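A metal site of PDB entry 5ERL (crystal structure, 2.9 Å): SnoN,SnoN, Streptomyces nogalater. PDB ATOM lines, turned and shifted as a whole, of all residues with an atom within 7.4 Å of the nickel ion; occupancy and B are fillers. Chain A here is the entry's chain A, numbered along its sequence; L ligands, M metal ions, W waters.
ND1 of His 225 sits at hydrogen-bond distance from O of Thr 223 (2.8 Å).
O of Ala 140 sits at hydrogen-bond distance from ND1 of His 142.
N of Asp 144 sits at hydrogen-bond distance from O of Ala 221 (3.5 Å).
Of the 18 residues printed, 3 come within 4 Å of the nickel ion.
O2 of LIG L1 binds the nickel ion (1.9 Å).
The nickel ion is bound by OD2 of Asp 144 (1.9 Å).
A ring nitrogen (NE2) of His 142 binds the nickel ion.
The nickel ion is bound by water W1 (2.0 Å).
NE2 of His 225 is bound to the nickel ion.
Slightly farther from the nickel ion lies OD1 of Asp 144 (2.8 Å).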
ATOM      1  N   TRP A  76     -28.905  -8.750 -13.934  1.00  0.00           N
ATOM      2  CA  TRP A  76     -28.252  -9.945 -14.341  1.00  0.00           C
ATOM      3  C   TRP A  76     -27.908 -10.579 -13.040  1.00  0.00           C
ATOM      4  O   TRP A  76     -27.163 -10.055 -12.277  1.00  0.00           O
ATOM      5  CB  TRP A  76     -27.026  -9.681 -15.180  1.00  0.00           C
ATOM      6  CG  TRP A  76     -26.053 -10.877 -15.392  1.00  0.00           C
ATOM      7  CD1 TRP A  76     -26.296 -12.202 -15.066  1.00  0.00           C
ATOM      8  CD2 TRP A  76     -24.771 -10.870 -16.067  1.00  0.00           C
ATOM      9  NE1 TRP A  76     -25.207 -12.982 -15.441  1.00  0.00           N
ATOM     10  CE2 TRP A  76     -24.281 -12.188 -16.041  1.00  0.00           C
ATOM     11  CE3 TRP A  76     -24.003  -9.873 -16.660  1.00  0.00           C
ATOM     12  CZ2 TRP A  76     -23.108 -12.548 -16.603  1.00  0.00           C
ATOM     13  CZ3 TRP A  76     -22.784 -10.239 -17.200  1.00  0.00           C
ATOM     14  CH2 TRP A  76     -22.361 -11.569 -17.172  1.00  0.00           C
ATOM     15  N   MET A  84     -24.701  -8.111 -11.606  1.00  0.00           N
ATOM     16  CA  MET A  84     -24.701  -6.641 -11.858  1.00  0.00           C
ATOM     17  C   MET A  84     -26.092  -6.153 -12.236  1.00  0.00           C
ATOM     18  O   MET A  84     -26.968  -6.947 -12.599  1.00  0.00           O
ATOM     19  CB  MET A  84     -23.758  -6.240 -12.967  1.00  0.00           C
ATOM     20  CG  MET A  84     -24.176  -6.848 -14.291  1.00  0.00           C
ATOM     21  SD  MET A  84     -23.072  -6.413 -15.648  1.00  0.00           S
ATOM     22  CE  MET A  84     -21.554  -7.322 -15.287  1.00  0.00           C
ATOM     23  N   THR A 139     -18.689 -11.938 -11.423  1.00  0.00           N
ATOM     24  CA  THR A 139     -19.082 -12.268 -12.800  1.00  0.00           C
ATOM     25  C   THR A 139     -18.325 -13.537 -13.156  1.00  0.00           C
ATOM     26  O   THR A 139     -17.105 -13.552 -13.168  1.00  0.00           O
ATOM     27  CB  THR A 139     -18.679 -11.227 -13.817  1.00  0.00           C
ATOM     28  OG1 THR A 139     -19.163  -9.943 -13.367  1.00  0.00           O
ATOM     29  CG2 THR A 139     -19.243 -11.522 -15.165  1.00  0.00           C
ATOM     30  N   ALA A 140     -19.046 -14.593 -13.431  1.00  0.00           N
ATOM     31  CA  ALA A 140     -18.375 -15.868 -13.613  1.00  0.00           C
ATOM     32  C   ALA A 140     -17.649 -15.896 -14.952  1.00  0.00           C
ATOM     33  O   ALA A 140     -17.968 -15.118 -15.822  1.00  0.00           O
ATOM     34  CB  ALA A 140     -19.362 -16.993 -13.477  1.00  0.00           C
ATOM     35  N   HIS A 142     -16.668 -16.516 -18.620  1.00  0.00           N
ATOM     36  CA  HIS A 142     -17.556 -16.663 -19.727  1.00  0.00           C
ATOM     37  C   HIS A 142     -16.864 -16.220 -20.997  1.00  0.00           C
ATOM     38  O   HIS A 142     -15.721 -15.943 -21.026  1.00  0.00           O
ATOM     39  CB  HIS A 142     -18.847 -15.887 -19.469  1.00  0.00           C
ATOM     40  CG  HIS A 142     -18.709 -14.413 -19.539  1.00  0.00           C
ATOM     41  ND1 HIS A 142     -18.181 -13.643 -18.541  1.00  0.00           N
ATOM     42  CD2 HIS A 142     -18.955 -13.586 -20.560  1.00  0.00           C
ATOM     43  CE1 HIS A 142     -18.179 -12.387 -18.930  1.00  0.00           C
ATOM     44  NE2 HIS A 142     -18.507 -12.350 -20.200  1.00  0.00           N
ATOM     45  N   HIS A 143     -17.611 -16.325 -22.064  1.00  0.00           N
ATOM     46  CA  HIS A 143     -17.127 -16.381 -23.458  1.00  0.00           C
ATOM     47  C   HIS A 143     -18.179 -15.592 -24.221  1.00  0.00           C
ATOM     48  O   HIS A 143     -19.133 -16.185 -24.744  1.00  0.00           O
ATOM     49  CB  HIS A 143     -17.151 -17.909 -23.966  1.00  0.00           C
ATOM     50  CG  HIS A 143     -16.398 -18.171 -25.231  1.00  0.00           C
ATOM     51  ND1 HIS A 143     -16.983 -18.129 -26.483  1.00  0.00           N
ATOM     52  CD2 HIS A 143     -15.098 -18.524 -25.432  1.00  0.00           C
ATOM     53  CE1 HIS A 143     -16.075 -18.428 -27.397  1.00  0.00           C
ATOM     54  NE2 HIS A 143     -14.919 -18.679 -26.795  1.00  0.00           N
ATOM     55  N   ASP A 144     -17.967 -14.310 -24.351  1.00  0.00           N
ATOM     56  CA  ASP A 144     -19.041 -13.414 -24.889  1.00  0.00           C
ATOM     57  C   ASP A 144     -19.489 -13.666 -26.330  1.00  0.00           C
ATOM     58  O   ASP A 144     -20.617 -13.447 -26.728  1.00  0.00           O
ATOM     59  CB  ASP A 144     -18.624 -11.925 -24.759  1.00  0.00           C
ATOM     60  CG  ASP A 144     -18.843 -11.370 -23.347  1.00  0.00           C
ATOM     61  OD1 ASP A 144     -19.952 -11.544 -22.823  1.00  0.00           O
ATOM     62  OD2 ASP A 144     -17.935 -10.660 -22.861  1.00  0.00           O
ATOM     63  N   ALA A 145     -18.615 -14.321 -27.063  1.00  0.00           N
ATOM     64  CA  ALA A 145     -18.692 -14.381 -28.507  1.00  0.00           C
ATOM     65  C   ALA A 145     -19.949 -14.775 -29.198  1.00  0.00           C
ATOM     66  O   ALA A 145     -20.418 -14.036 -30.013  1.00  0.00           O
ATOM     67  CB  ALA A 145     -17.522 -15.185 -29.071  1.00  0.00           C
ATOM     68  N   PHE A 148     -23.603 -12.718 -29.057  1.00  0.00           N
ATOM     69  CA  PHE A 148     -23.858 -11.504 -29.841  1.00  0.00           C
ATOM     70  C   PHE A 148     -24.659 -11.916 -31.052  1.00  0.00           C
ATOM     71  O   PHE A 148     -24.201 -12.746 -31.804  1.00  0.00           O
ATOM     72  CB  PHE A 148     -22.549 -10.862 -30.318  1.00  0.00           C
ATOM     73  CG  PHE A 148     -21.703 -10.305 -29.190  1.00  0.00           C
ATOM     74  CD1 PHE A 148     -22.228  -9.643 -28.152  1.00  0.00           C
ATOM     75  CD2 PHE A 148     -20.343 -10.501 -29.199  1.00  0.00           C
ATOM     76  CE1 PHE A 148     -21.434  -9.212 -27.125  1.00  0.00           C
ATOM     77  CE2 PHE A 148     -19.543 -10.021 -28.187  1.00  0.00           C
ATOM     78  CZ  PHE A 148     -20.096  -9.396 -27.153  1.00  0.00           C
ATOM     79  N   THR A 158     -14.932  -5.656 -27.509  1.00  0.00           N
ATOM     80  CA  THR A 158     -15.630  -5.020 -26.450  1.00  0.00           C
ATOM     81  C   THR A 158     -14.653  -4.064 -25.751  1.00  0.00           C
ATOM     82  O   THR A 158     -13.527  -4.455 -25.409  1.00  0.00           O
ATOM     83  CB  THR A 158     -16.018  -6.001 -25.377  1.00  0.00           C
ATOM     84  OG1 THR A 158     -16.907  -7.088 -25.867  1.00  0.00           O
ATOM     85  CG2 THR A 158     -16.688  -5.299 -24.278  1.00  0.00           C
ATOM     86  N   TRP A 160     -14.291  -1.734 -22.432  1.00  0.00           N
ATOM     87  CA  TRP A 160     -14.794  -1.585 -21.064  1.00  0.00           C
ATOM     88  C   TRP A 160     -14.072  -0.423 -20.382  1.00  0.00           C
ATOM     89  O   TRP A 160     -12.821  -0.480 -20.212  1.00  0.00           O
ATOM     90  CB  TRP A 160     -14.498  -2.806 -20.285  1.00  0.00           C
ATOM     91  CG  TRP A 160     -15.236  -3.061 -19.074  1.00  0.00           C
ATOM     92  CD1 TRP A 160     -16.202  -4.028 -18.940  1.00  0.00           C
ATOM     93  CD2 TRP A 160     -14.969  -2.585 -17.773  1.00  0.00           C
ATOM     94  NE1 TRP A 160     -16.534  -4.155 -17.623  1.00  0.00           N
ATOM     95  CE2 TRP A 160     -15.837  -3.201 -16.910  1.00  0.00           C
ATOM     96  CE3 TRP A 160     -14.061  -1.712 -17.244  1.00  0.00           C
ATOM     97  CZ2 TRP A 160     -15.854  -2.936 -15.524  1.00  0.00           C
ATOM     98  CZ3 TRP A 160     -14.086  -1.457 -15.850  1.00  0.00           C
ATOM     99  CH2 TRP A 160     -14.976  -2.090 -15.027  1.00  0.00           C
ATOM    100  N   MET A 173     -11.722  -6.888 -13.742  1.00  0.00           N
ATOM    101  CA  MET A 173     -11.796  -8.090 -14.542  1.00  0.00           C
ATOM    102  C   MET A 173     -10.568  -8.943 -14.422  1.00  0.00           C
ATOM    103  O   MET A 173      -9.538  -8.492 -14.002  1.00  0.00           O
ATOM    104  CB  MET A 173     -12.114  -7.745 -16.005  1.00  0.00           C
ATOM    105  CG  MET A 173     -13.638  -7.762 -16.261  1.00  0.00           C
ATOM    106  SD  MET A 173     -14.183  -7.530 -17.973  1.00  0.00           S
ATOM    107  CE  MET A 173     -13.553  -5.820 -17.998  1.00  0.00           C
ATOM    108  N   HIS A 219     -11.188  -6.114 -25.176  1.00  0.00           N
ATOM    109  CA  HIS A 219     -11.033  -7.601 -25.335  1.00  0.00           C
ATOM    110  C   HIS A 219     -11.800  -8.198 -26.423  1.00  0.00           C
ATOM    111  O   HIS A 219     -12.945  -7.824 -26.726  1.00  0.00           O
ATOM    112  CB  HIS A 219     -11.296  -8.395 -24.050  1.00  0.00           C
ATOM    113  CG  HIS A 219     -12.747  -8.412 -23.617  1.00  0.00           C
ATOM    114  ND1 HIS A 219     -13.294  -7.438 -22.811  1.00  0.00           N
ATOM    115  CD2 HIS A 219     -13.762  -9.237 -23.905  1.00  0.00           C
ATOM    116  CE1 HIS A 219     -14.579  -7.723 -22.585  1.00  0.00           C
ATOM    117  NE2 HIS A 219     -14.876  -8.802 -23.242  1.00  0.00           N
ATOM    118  N   ALA A 221     -13.801 -10.993 -28.538  1.00  0.00           N
ATOM    119  CA  ALA A 221     -15.071 -11.764 -28.230  1.00  0.00           C
ATOM    120  C   ALA A 221     -14.859 -13.147 -27.662  1.00  0.00           C
ATOM    121  O   ALA A 221     -15.498 -13.561 -26.685  1.00  0.00           O
ATOM    122  CB  ALA A 221     -15.945 -11.873 -29.446  1.00  0.00           C
ATOM    123  N   THR A 223     -12.127 -14.124 -26.044  1.00  0.00           N
ATOM    124  CA  THR A 223     -11.256 -14.146 -24.878  1.00  0.00           C
ATOM    125  C   THR A 223     -12.102 -14.517 -23.660  1.00  0.00           C
ATOM    126  O   THR A 223     -13.136 -13.877 -23.378  1.00  0.00           O
ATOM    127  CB  THR A 223     -10.552 -12.795 -24.664  1.00  0.00           C
ATOM    128  OG1 THR A 223      -9.764 -12.505 -25.803  1.00  0.00           O
ATOM    129  CG2 THR A 223      -9.680 -12.827 -23.484  1.00  0.00           C
ATOM    130  N   HIS A 225     -12.940 -14.380 -19.926  1.00  0.00           N
ATOM    131  CA  HIS A 225     -12.749 -13.392 -18.871  1.00  0.00           C
ATOM    132  C   HIS A 225     -13.824 -13.502 -17.809  1.00  0.00           C
ATOM    133  O   HIS A 225     -14.843 -14.072 -18.017  1.00  0.00           O
ATOM    134  CB  HIS A 225     -12.728 -11.939 -19.447  1.00  0.00           C
ATOM    135  CG  HIS A 225     -13.965 -11.599 -20.209  1.00  0.00           C
ATOM    136  ND1 HIS A 225     -14.275 -12.139 -21.433  1.00  0.00           N
ATOM    137  CD2 HIS A 225     -15.069 -10.938 -19.818  1.00  0.00           C
ATOM    138  CE1 HIS A 225     -15.491 -11.766 -21.791  1.00  0.00           C
ATOM    139  NE2 HIS A 225     -16.042 -11.101 -20.786  1.00  0.00           N
ATOM    140  N   SER A 226     -13.565 -12.875 -16.685  1.00  0.00           N
ATOM    141  CA  SER A 226     -14.387 -12.948 -15.484  1.00  0.00           C
ATOM    142  C   SER A 226     -14.214 -11.618 -14.725  1.00  0.00           C
ATOM    143  O   SER A 226     -13.459 -10.748 -15.160  1.00  0.00           O
ATOM    144  CB  SER A 226     -13.913 -14.111 -14.614  1.00  0.00           C
ATOM    145  OG  SER A 226     -12.779 -13.699 -13.843  1.00  0.00           O
ATOM    146  N   SER A 240     -19.645  -0.648 -20.961  1.00  0.00           N
ATOM    147  CA  SER A 240     -19.182  -1.733 -21.856  1.00  0.00           C
ATOM    148  C   SER A 240     -19.803  -1.557 -23.203  1.00  0.00           C
ATOM    149  O   SER A 240     -20.982  -1.589 -23.332  1.00  0.00           O
ATOM    150  CB  SER A 240     -19.592  -3.113 -21.310  1.00  0.00           C
ATOM    151  OG  SER A 240     -18.891  -4.157 -21.965  1.00  0.00           O
HETATM  152  C1  LIG L   1     -18.040  -8.198 -19.690  1.00  0.00           C
HETATM  153  O1  LIG L   1     -18.158  -7.452 -20.870  1.00  0.00           O
HETATM  154  O2  LIG L   1     -18.221  -9.531 -19.379  1.00  0.00           O
HETATM  155  C2  LIG L   1     -17.704  -7.527 -18.284  1.00  0.00           C
HETATM  156  C3  LIG L   1     -18.569  -8.139 -17.064  1.00  0.00           C
HETATM  157  C4  LIG L   1     -18.314  -7.387 -15.704  1.00  0.00           C
HETATM  158  O3  LIG L   1     -18.229  -5.996 -15.704  1.00  0.00           O
HETATM  159  O4  LIG L   1     -18.112  -8.156 -14.634  1.00  0.00           O
HETATM  160  C1  LG2 L   2     -24.333 -19.766 -14.924  1.00  0.00           C
HETATM  161  C2  LG2 L   2     -24.228 -20.662 -13.736  1.00  0.00           C
HETATM  162  O1  LG2 L   2     -25.582 -21.230 -13.466  1.00  0.00           O
HETATM  163  C3  LG2 L   2     -23.496 -19.665 -12.571  1.00  0.00           C
HETATM  164  O2  LG2 L   2     -22.130 -19.152 -13.027  1.00  0.00           O
HETATM  165  C4  LG2 L   2     -24.397 -18.415 -12.082  1.00  0.00           C
HETATM  166  C5  LG2 L   2     -25.673 -18.905 -11.281  1.00  0.00           C
HETATM  167  O3  LG2 L   2     -24.685 -17.585 -13.276  1.00  0.00           O
HETATM  168  C6  LG2 L   2     -25.210 -18.560 -14.474  1.00  0.00           C
HETATM  169  O4  LG2 L   2     -25.424 -17.881 -15.657  1.00  0.00           O
HETATM  170  C7  LG2 L   2     -26.728 -17.331 -15.811  1.00  0.00           C
HETATM  171  C8  LG2 L   2     -27.651 -17.005 -14.546  1.00  0.00           C
HETATM  172  C9  LG2 L   2     -29.043 -16.773 -15.110  1.00  0.00           C
HETATM  173  C10 LG2 L   2     -30.188 -16.581 -14.074  1.00  0.00           C
HETATM  174  O5  LG2 L   2     -29.241 -17.955 -15.716  1.00  0.00           O
HETATM  175  C11 LG2 L   2     -26.628 -16.206 -16.654  1.00  0.00           C
HETATM  176  C12 LG2 L   2     -25.454 -15.842 -17.379  1.00  0.00           C
HETATM  177  O6  LG2 L   2     -24.321 -16.521 -17.289  1.00  0.00           O
HETATM  178  C13 LG2 L   2     -25.375 -14.816 -18.277  1.00  0.00           C
HETATM  179  C14 LG2 L   2     -24.185 -14.585 -18.961  1.00  0.00           C
HETATM  180  O7  LG2 L   2     -23.205 -15.291 -18.745  1.00  0.00           O
HETATM  181  C15 LG2 L   2     -24.180 -13.458 -19.863  1.00  0.00           C
HETATM  182  C16 LG2 L   2     -23.060 -13.157 -20.610  1.00  0.00           C
HETATM  183  O8  LG2 L   2     -21.973 -13.939 -20.429  1.00  0.00           O
HETATM  184  C17 LG2 L   2     -23.057 -12.090 -21.469  1.00  0.00           C
HETATM  185  C18 LG2 L   2     -24.167 -11.275 -21.697  1.00  0.00           C
HETATM  186  C19 LG2 L   2     -24.180 -10.096 -22.683  1.00  0.00           C
HETATM  187  C20 LG2 L   2     -23.644 -10.633 -24.056  1.00  0.00           C
HETATM  188  O9  LG2 L   2     -25.391  -9.522 -23.048  1.00  0.00           O
HETATM  189  C21 LG2 L   2     -23.460  -8.976 -22.200  1.00  0.00           C
HETATM  190  O10 LG2 L   2     -23.164  -8.063 -23.247  1.00  0.00           O
HETATM  191  C22 LG2 L   2     -24.255  -8.487 -21.007  1.00  0.00           C
HETATM  192  N1  LG2 L   2     -23.799  -7.209 -20.455  1.00  0.00           N
HETATM  193  C23 LG2 L   2     -24.603  -6.770 -19.276  1.00  0.00           C
HETATM  194  C24 LG2 L   2     -22.363  -7.139 -20.159  1.00  0.00           C
HETATM  195  C25 LG2 L   2     -25.782  -8.524 -21.263  1.00  0.00           C
HETATM  196  C26 LG2 L   2     -26.249  -9.572 -22.042  1.00  0.00           C
HETATM  197  O11 LG2 L   2     -26.373 -10.804 -21.167  1.00  0.00           O
HETATM  198  C27 LG2 L   2     -25.279 -11.607 -20.966  1.00  0.00           C
HETATM  199  C28 LG2 L   2     -25.323 -12.648 -20.065  1.00  0.00           C
HETATM  200  C29 LG2 L   2     -26.506 -12.910 -19.346  1.00  0.00           C
HETATM  201  O12 LG2 L   2     -27.502 -12.221 -19.496  1.00  0.00           O
HETATM  202  C30 LG2 L   2     -26.518 -14.026 -18.450  1.00  0.00           C
HETATM  203  C31 LG2 L   2     -27.697 -14.379 -17.718  1.00  0.00           C
HETATM  204  C32 LG2 L   2     -27.820 -15.460 -16.822  1.00  0.00           C
HETATM  205  C33 LG2 L   2     -29.104 -15.710 -16.183  1.00  0.00           C
HETATM  206  C34 LG2 L   2     -30.091 -16.254 -17.129  1.00  0.00           C
HETATM  207  O13 LG2 L   2     -31.321 -16.176 -17.044  1.00  0.00           O
HETATM  208  O14 LG2 L   2     -29.513 -17.195 -18.067  1.00  0.00           O
HETATM  209  C35 LG2 L   2     -30.420 -17.601 -19.158  1.00  0.00           C
HETATM  210 NI    NI M   1     -18.088 -10.581 -20.924  1.00  0.00          NI
HETATM  211  O   HOH W   1     -20.024 -10.176 -20.977  1.00  0.00           O
